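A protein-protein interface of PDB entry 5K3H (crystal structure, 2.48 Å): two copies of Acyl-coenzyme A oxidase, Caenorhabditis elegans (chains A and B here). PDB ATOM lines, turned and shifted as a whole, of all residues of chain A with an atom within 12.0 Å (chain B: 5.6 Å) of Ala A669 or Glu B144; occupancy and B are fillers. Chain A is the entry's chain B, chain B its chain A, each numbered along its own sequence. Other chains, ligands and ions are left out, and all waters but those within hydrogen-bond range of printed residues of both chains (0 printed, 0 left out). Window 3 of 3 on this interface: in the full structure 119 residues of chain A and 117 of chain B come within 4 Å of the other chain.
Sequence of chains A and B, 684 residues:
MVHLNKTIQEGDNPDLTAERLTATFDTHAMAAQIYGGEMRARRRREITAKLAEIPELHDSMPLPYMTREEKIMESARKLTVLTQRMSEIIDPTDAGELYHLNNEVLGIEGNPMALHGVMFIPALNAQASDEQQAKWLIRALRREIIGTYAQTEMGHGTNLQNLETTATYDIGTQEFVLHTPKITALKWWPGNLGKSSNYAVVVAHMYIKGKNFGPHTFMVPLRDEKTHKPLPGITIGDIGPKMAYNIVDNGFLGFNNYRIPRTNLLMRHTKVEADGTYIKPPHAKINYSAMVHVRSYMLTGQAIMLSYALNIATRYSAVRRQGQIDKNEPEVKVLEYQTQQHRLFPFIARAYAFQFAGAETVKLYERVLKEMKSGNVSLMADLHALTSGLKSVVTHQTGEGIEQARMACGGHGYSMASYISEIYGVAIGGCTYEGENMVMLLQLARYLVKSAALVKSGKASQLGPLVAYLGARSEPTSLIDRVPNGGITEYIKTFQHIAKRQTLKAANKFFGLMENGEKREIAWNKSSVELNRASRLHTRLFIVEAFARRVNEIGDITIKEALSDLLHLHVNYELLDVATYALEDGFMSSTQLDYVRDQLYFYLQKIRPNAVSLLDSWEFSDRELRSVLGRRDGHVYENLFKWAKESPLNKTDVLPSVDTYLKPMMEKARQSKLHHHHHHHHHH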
ATOM      1  N   VAL A 658     -18.746  10.056   3.144  1.00  0.00           N
ATOM      2  CA  VAL A 658     -19.029  11.314   2.459  1.00  0.00           C
ATOM      3  C   VAL A 658     -19.153  12.470   3.451  1.00  0.00           C
ATOM      4  O   VAL A 658     -18.689  13.583   3.176  1.00  0.00           O
ATOM      5  CB  VAL A 658     -20.288  11.170   1.580  1.00  0.00           C
ATOM      6  CG1 VAL A 658     -20.619  12.484   0.911  1.00  0.00           C
ATOM      7  CG2 VAL A 658     -20.070  10.089   0.508  1.00  0.00           C
ATOM      8  N   TYR A 661     -15.249  12.568   5.253  1.00  0.00           N
ATOM      9  CA  TYR A 661     -14.260  12.859   4.235  1.00  0.00           C
ATOM     10  C   TYR A 661     -15.002  13.186   2.953  1.00  0.00           C
ATOM     11  O   TYR A 661     -16.226  13.301   2.944  1.00  0.00           O
ATOM     12  CB  TYR A 661     -13.314  11.674   4.040  1.00  0.00           C
ATOM     13  CG  TYR A 661     -12.734  11.069   5.316  1.00  0.00           C
ATOM     14  CD1 TYR A 661     -11.779  11.744   6.061  1.00  0.00           C
ATOM     15  CD2 TYR A 661     -13.119   9.807   5.743  1.00  0.00           C
ATOM     16  CE1 TYR A 661     -11.237  11.191   7.198  1.00  0.00           C
ATOM     17  CE2 TYR A 661     -12.583   9.244   6.879  1.00  0.00           C
ATOM     18  CZ  TYR A 661     -11.633   9.935   7.606  1.00  0.00           C
ATOM     19  OH  TYR A 661     -11.082   9.375   8.753  1.00  0.00           O
ATOM     20  N   LEU A 662     -14.267  13.390   1.868  1.00  0.00           N
ATOM     21  CA  LEU A 662     -14.928  13.454   0.564  1.00  0.00           C
ATOM     22  C   LEU A 662     -15.727  14.738   0.365  1.00  0.00           C
ATOM     23  O   LEU A 662     -15.395  15.531  -0.522  1.00  0.00           O
ATOM     24  CB  LEU A 662     -15.830  12.224   0.334  1.00  0.00           C
ATOM     25  CG  LEU A 662     -15.277  11.090  -0.540  1.00  0.00           C
ATOM     26  CD1 LEU A 662     -13.836  10.743  -0.177  1.00  0.00           C
ATOM     27  CD2 LEU A 662     -16.174   9.855  -0.436  1.00  0.00           C
ATOM     28  N   LYS A 663     -16.799  14.959   1.132  1.00  0.00           N
ATOM     29  CA  LYS A 663     -17.476  16.247   0.986  1.00  0.00           C
ATOM     30  C   LYS A 663     -16.669  17.370   1.624  1.00  0.00           C
ATOM     31  O   LYS A 663     -16.476  18.407   0.967  1.00  0.00           O
ATOM     32  CB  LYS A 663     -18.924  16.161   1.471  1.00  0.00           C
ATOM     33  CG  LYS A 663     -19.754  17.395   1.103  1.00  0.00           C
ATOM     34  CD  LYS A 663     -21.207  17.217   1.536  1.00  0.00           C
ATOM     35  CE  LYS A 663     -21.399  17.387   3.041  1.00  0.00           C
ATOM     36  NZ  LYS A 663     -22.848  17.284   3.412  1.00  0.00           N
ATOM     37  N   PRO A 664     -16.157  17.247   2.856  1.00  0.00           N
ATOM     38  CA  PRO A 664     -15.153  18.230   3.296  1.00  0.00           C
ATOM     39  C   PRO A 664     -14.043  18.426   2.276  1.00  0.00           C
ATOM     40  O   PRO A 664     -13.645  19.568   2.001  1.00  0.00           O
ATOM     41  CB  PRO A 664     -14.627  17.622   4.609  1.00  0.00           C
ATOM     42  CG  PRO A 664     -15.815  16.868   5.162  1.00  0.00           C
ATOM     43  CD  PRO A 664     -16.526  16.313   3.944  1.00  0.00           C
ATOM     44  N   MET A 665     -13.571  17.334   1.667  1.00  0.00           N
ATOM     45  CA  MET A 665     -12.527  17.437   0.656  1.00  0.00           C
ATOM     46  C   MET A 665     -12.969  18.288  -0.528  1.00  0.00           C
ATOM     47  O   MET A 665     -12.197  19.109  -1.037  1.00  0.00           O
ATOM     48  CB  MET A 665     -12.131  16.040   0.182  1.00  0.00           C
ATOM     49  CG  MET A 665     -11.151  16.020  -0.983  1.00  0.00           C
ATOM     50  SD  MET A 665     -11.220  14.408  -1.789  1.00  0.00           S
ATOM     51  CE  MET A 665     -12.844  14.490  -2.551  1.00  0.00           C
ATOM     52  N   MET A 666     -14.201  18.096  -0.994  1.00  0.00           N
ATOM     53  CA  MET A 666     -14.666  18.858  -2.147  1.00  0.00           C
ATOM     54  C   MET A 666     -14.875  20.326  -1.788  1.00  0.00           C
ATOM     55  O   MET A 666     -14.434  21.223  -2.520  1.00  0.00           O
ATOM     56  CB  MET A 666     -15.958  18.248  -2.698  1.00  0.00           C
ATOM     57  CG  MET A 666     -15.770  16.952  -3.475  1.00  0.00           C
ATOM     58  SD  MET A 666     -17.323  16.393  -4.241  1.00  0.00           S
ATOM     59  CE  MET A 666     -18.215  15.798  -2.786  1.00  0.00           C
ATOM     60  N   GLU A 667     -15.527  20.584  -0.648  1.00  0.00           N
ATOM     61  CA  GLU A 667     -15.782  21.953  -0.204  1.00  0.00           C
ATOM     62  C   GLU A 667     -14.489  22.754  -0.114  1.00  0.00           C
ATOM     63  O   GLU A 667     -14.422  23.898  -0.590  1.00  0.00           O
ATOM     64  CB  GLU A 667     -16.529  21.926   1.136  1.00  0.00           C
ATOM     65  CG  GLU A 667     -18.066  21.804   0.981  1.00  0.00           C
ATOM     66  CD  GLU A 667     -18.764  21.088   2.156  1.00  0.00           C
ATOM     67  OE1 GLU A 667     -19.967  20.750   2.010  1.00  0.00           O
ATOM     68  OE2 GLU A 667     -18.131  20.871   3.223  1.00  0.00           O
ATOM     69  N   LYS A 668     -13.438  22.145   0.440  1.00  0.00           N
ATOM     70  CA  LYS A 668     -12.151  22.821   0.582  1.00  0.00           C
ATOM     71  C   LYS A 668     -11.589  23.274  -0.768  1.00  0.00           C
ATOM     72  O   LYS A 668     -10.873  24.281  -0.842  1.00  0.00           O
ATOM     73  CB  LYS A 668     -11.188  21.855   1.279  1.00  0.00           C
ATOM     74  CG  LYS A 668      -9.822  22.383   1.674  1.00  0.00           C
ATOM     75  CD  LYS A 668      -9.012  21.226   2.270  1.00  0.00           C
ATOM     76  CE  LYS A 668      -7.574  21.612   2.611  1.00  0.00           C
ATOM     77  NZ  LYS A 668      -6.801  20.429   3.132  1.00  0.00           N
ATOM     78  N   ALA A 669     -11.943  22.588  -1.848  1.00  0.00           N
ATOM     79  CA  ALA A 669     -11.403  22.913  -3.158  1.00  0.00           C
ATOM     80  C   ALA A 669     -12.308  23.933  -3.819  1.00  0.00           C
ATOM     81  O   ALA A 669     -13.345  24.284  -3.263  1.00  0.00           O
ATOM     82  CB  ALA A 669     -11.272  21.661  -4.020  1.00  0.00           C
ATOM     83  N   ILE B 138     -12.531  21.521 -15.258  1.00  0.00           N
ATOM     84  CA  ILE B 138     -11.656  22.108 -14.240  1.00  0.00           C
ATOM     85  C   ILE B 138     -12.136  21.749 -12.841  1.00  0.00           C
ATOM     86  O   ILE B 138     -11.331  21.407 -11.963  1.00  0.00           O
ATOM     87  CB  ILE B 138     -11.562  23.635 -14.417  1.00  0.00           C
ATOM     88  CG1 ILE B 138     -10.900  23.981 -15.744  1.00  0.00           C
ATOM     89  CG2 ILE B 138     -10.802  24.252 -13.261  1.00  0.00           C
ATOM     90  CD1 ILE B 138      -9.554  23.342 -15.893  1.00  0.00           C
ATOM     91  N   ARG B 139     -13.449  21.835 -12.604  1.00  0.00           N
ATOM     92  CA  ARG B 139     -13.979  21.452 -11.298  1.00  0.00           C
ATOM     93  C   ARG B 139     -13.665  19.988 -10.990  1.00  0.00           C
ATOM     94  O   ARG B 139     -13.359  19.635  -9.845  1.00  0.00           O
ATOM     95  CB  ARG B 139     -15.493  21.690 -11.243  1.00  0.00           C
ATOM     96  CG  ARG B 139     -15.973  23.130 -11.348  1.00  0.00           C
ATOM     97  CD  ARG B 139     -17.439  23.202 -10.897  1.00  0.00           C
ATOM     98  NE  ARG B 139     -17.575  23.061  -9.447  1.00  0.00           N
ATOM     99  CZ  ARG B 139     -18.683  22.662  -8.818  1.00  0.00           C
ATOM    100  NH1 ARG B 139     -19.765  22.333  -9.513  1.00  0.00           N
ATOM    101  NH2 ARG B 139     -18.707  22.574  -7.488  1.00  0.00           N
ATOM    102  N   ALA B 140     -13.742  19.125 -12.005  1.00  0.00           N
ATOM    103  CA  ALA B 140     -13.408  17.719 -11.808  1.00  0.00           C
ATOM    104  C   ALA B 140     -11.922  17.544 -11.515  1.00  0.00           C
ATOM    105  O   ALA B 140     -11.546  16.822 -10.582  1.00  0.00           O
ATOM    106  CB  ALA B 140     -13.815  16.906 -13.038  1.00  0.00           C
ATOM    107  N   ARG B 142      -9.886  19.597 -10.226  1.00  0.00           N
ATOM    108  CA  ARG B 142      -9.615  20.132  -8.898  1.00  0.00           C
ATOM    109  C   ARG B 142     -10.329  19.349  -7.807  1.00  0.00           C
ATOM    110  O   ARG B 142     -10.147  19.656  -6.625  1.00  0.00           O
ATOM    111  CB  ARG B 142     -10.047  21.598  -8.850  1.00  0.00           C
ATOM    112  CG  ARG B 142      -9.224  22.545  -9.730  1.00  0.00           C
ATOM    113  CD  ARG B 142      -9.904  23.914  -9.784  1.00  0.00           C
ATOM    114  NE  ARG B 142     -10.122  24.450  -8.443  1.00  0.00           N
ATOM    115  CZ  ARG B 142      -9.205  25.099  -7.738  1.00  0.00           C
ATOM    116  NH1 ARG B 142      -8.005  25.315  -8.257  1.00  0.00           N
ATOM    117  NH2 ARG B 142      -9.493  25.537  -6.516  1.00  0.00           N
ATOM    118  N   ARG B 143     -11.127  18.350  -8.191  1.00  0.00           N
ATOM    119  CA  ARG B 143     -11.842  17.468  -7.273  1.00  0.00           C
ATOM    120  C   ARG B 143     -12.865  18.225  -6.437  1.00  0.00           C
ATOM    121  O   ARG B 143     -13.128  17.880  -5.279  1.00  0.00           O
ATOM    122  CB  ARG B 143     -10.873  16.668  -6.396  1.00  0.00           C
ATOM    123  CG  ARG B 143      -9.858  15.884  -7.230  1.00  0.00           C
ATOM    124  CD  ARG B 143      -8.977  14.986  -6.389  1.00  0.00           C
ATOM    125  NE  ARG B 143      -8.488  13.852  -7.174  1.00  0.00           N
ATOM    126  CZ  ARG B 143      -7.410  13.132  -6.869  1.00  0.00           C
ATOM    127  NH1 ARG B 143      -6.697  13.423  -5.798  1.00  0.00           N
ATOM    128  NH2 ARG B 143      -7.039  12.122  -7.639  1.00  0.00           N
ATOM    129  N   GLU B 144     -13.452  19.272  -7.024  1.00  0.00           N
ATOM    130  CA  GLU B 144     -14.599  19.917  -6.394  1.00  0.00           C
ATOM    131  C   GLU B 144     -15.845  19.055  -6.506  1.00  0.00           C
ATOM    132  O   GLU B 144     -16.761  19.183  -5.684  1.00  0.00           O
ATOM    133  CB  GLU B 144     -14.873  21.278  -7.036  1.00  0.00           C
ATOM    134  CG  GLU B 144     -13.737  22.258  -6.940  1.00  0.00           C
ATOM    135  CD  GLU B 144     -14.064  23.576  -7.605  1.00  0.00           C
ATOM    136  OE1 GLU B 144     -15.264  23.910  -7.685  1.00  0.00           O
ATOM    137  OE2 GLU B 144     -13.125  24.251  -8.086  1.00  0.00           O
ATOM    138  N   ILE B 145     -15.879  18.164  -7.498  1.00  0.00           N
ATOM    139  CA  ILE B 145     -16.984  17.246  -7.713  1.00  0.00           C
ATOM    140  C   ILE B 145     -16.401  15.853  -7.912  1.00  0.00           C
ATOM    141  O   ILE B 145     -15.208  15.679  -8.186  1.00  0.00           O
ATOM    142  CB  ILE B 145     -17.866  17.663  -8.910  1.00  0.00           C
ATOM    143  CG1 ILE B 145     -17.045  17.784 -10.200  1.00  0.00           C
ATOM    144  CG2 ILE B 145     -18.594  18.960  -8.603  1.00  0.00           C
ATOM    145  CD1 ILE B 145     -17.894  18.114 -11.440  1.00  0.00           C
ATOM    146  N   ILE B 146     -17.253  14.853  -7.718  1.00  0.00           N
ATOM    147  CA  ILE B 146     -16.893  13.453  -7.917  1.00  0.00           C
ATOM    148  C   ILE B 146     -17.825  12.915  -8.994  1.00  0.00           C
ATOM    149  O   ILE B 146     -19.054  13.009  -8.869  1.00  0.00           O
ATOM    150  CB  ILE B 146     -16.990  12.630  -6.616  1.00  0.00           C
ATOM    151  CG1 ILE B 146     -16.051  13.181  -5.539  1.00  0.00           C
ATOM    152  CG2 ILE B 146     -16.640  11.169  -6.866  1.00  0.00           C
ATOM    153  CD1 ILE B 146     -16.167  12.481  -4.206  1.00  0.00           C
ATOM    154  N   ASN B 198     -21.556  12.898  -7.195  1.00  0.00           N
ATOM    155  CA  ASN B 198     -22.675  13.823  -7.332  1.00  0.00           C
ATOM    156  C   ASN B 198     -22.927  14.236  -8.776  1.00  0.00           C
ATOM    157  O   ASN B 198     -23.974  14.828  -9.056  1.00  0.00           O
ATOM    158  CB  ASN B 198     -22.484  15.070  -6.444  1.00  0.00           C
ATOM    159  CG  ASN B 198     -21.070  15.661  -6.503  1.00  0.00           C
ATOM    160  OD1 ASN B 198     -20.316  15.488  -7.474  1.00  0.00           O
ATOM    161  ND2 ASN B 198     -20.698  16.340  -5.429  1.00  0.00           N
ATOM    162  N   GLU B 225     -25.045  19.504  -4.113  1.00  0.00           N
ATOM    163  CA  GLU B 225     -23.646  19.688  -3.733  1.00  0.00           C
ATOM    164  C   GLU B 225     -23.484  20.057  -2.270  1.00  0.00           C
ATOM    165  O   GLU B 225     -22.389  19.918  -1.725  1.00  0.00           O
ATOM    166  CB  GLU B 225     -22.991  20.777  -4.574  1.00  0.00           C
ATOM    167  CG  GLU B 225     -22.967  20.504  -6.055  1.00  0.00           C
ATOM    168  CD  GLU B 225     -21.855  21.260  -6.755  1.00  0.00           C
ATOM    169  OE1 GLU B 225     -20.946  21.746  -6.050  1.00  0.00           O
ATOM    170  OE2 GLU B 225     -21.893  21.388  -8.001  1.00  0.00           O
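SD of Met A666 is in hydrogen-bond range of ND2 of Asn B198 (3.6 Å).
SD of Met A666 sits close to O of Glu B144 (3.2 Å).
The guanidinium group (NE) of Arg B139 is in salt-bridge range of the side-chain carboxylate (OE1) of Glu B144 (3.0 Å).
NE of Arg B142 is in salt-bridge range of OE2 of Glu B144 (3.0 Å).
The backbone NH (N) of Asn B198 sits at hydrogen-bond distance from the backbone carbonyl oxygen (O) of Ile B146 (3.0 Å).
Among the printed residues, pairs that only touch across the chains: Met A666 with Arg B143, Ala A669 with Arg B142, Met A666 with Ile B145, Met A666 with Ile B146 and Ala A669 with Glu B144.
Hydrophobic or aromatic side chains of chain A within 4 Å of the printed part of chain B: Met A666 and Ala A669.
Among the printed residues, 7 pairs touch across the chains.
Among the printed residues, no Asp or Glu carboxylate lies within 4 Å of a Lys or Arg side-chain nitrogen of the other chain.
No position is printed for both chains.
Of the 7 pairs that touch across the chains among the printed residues, none has its exchanged pair printed and touching as well.
Ala A669 touches just these residues of chain B: Arg B142 (3.5 Å) and Glu B144 (3.8 Å).
Of chain A, only Met A666 (3.2 Å) and Ala A669 (3.8 Å) come within 4 Å of Glu B144.
No residue of chain A comes within 4 Å of Arg B139.
Arg B142 touches just one residue of chain A: Ala A669 (3.5 Å).
Ile B145 touches one residue of chain A.
Ile B146 touches just one residue of chain A: Met A666 (3.7 Å).
Of the printed residues of chain A, Asn B198 touches Met A666 (3.6 Å).
Of the printed residues of chain A, Arg B143 touches Met A666 (3.3 Å).
Printed residues of chain B within 4 Å of Met A666: Arg B143 (3.3 Å), Glu B144 (3.2 Å), Ile B145 (3.6 Å), Ile B146 (3.7 Å) and Asn B198 (3.6 Å).
Val A658 touches none of the printed residues of chain B.
The nearest printed residue of chain A that does not touch Arg B143 is Met A665 (4.4 Å).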
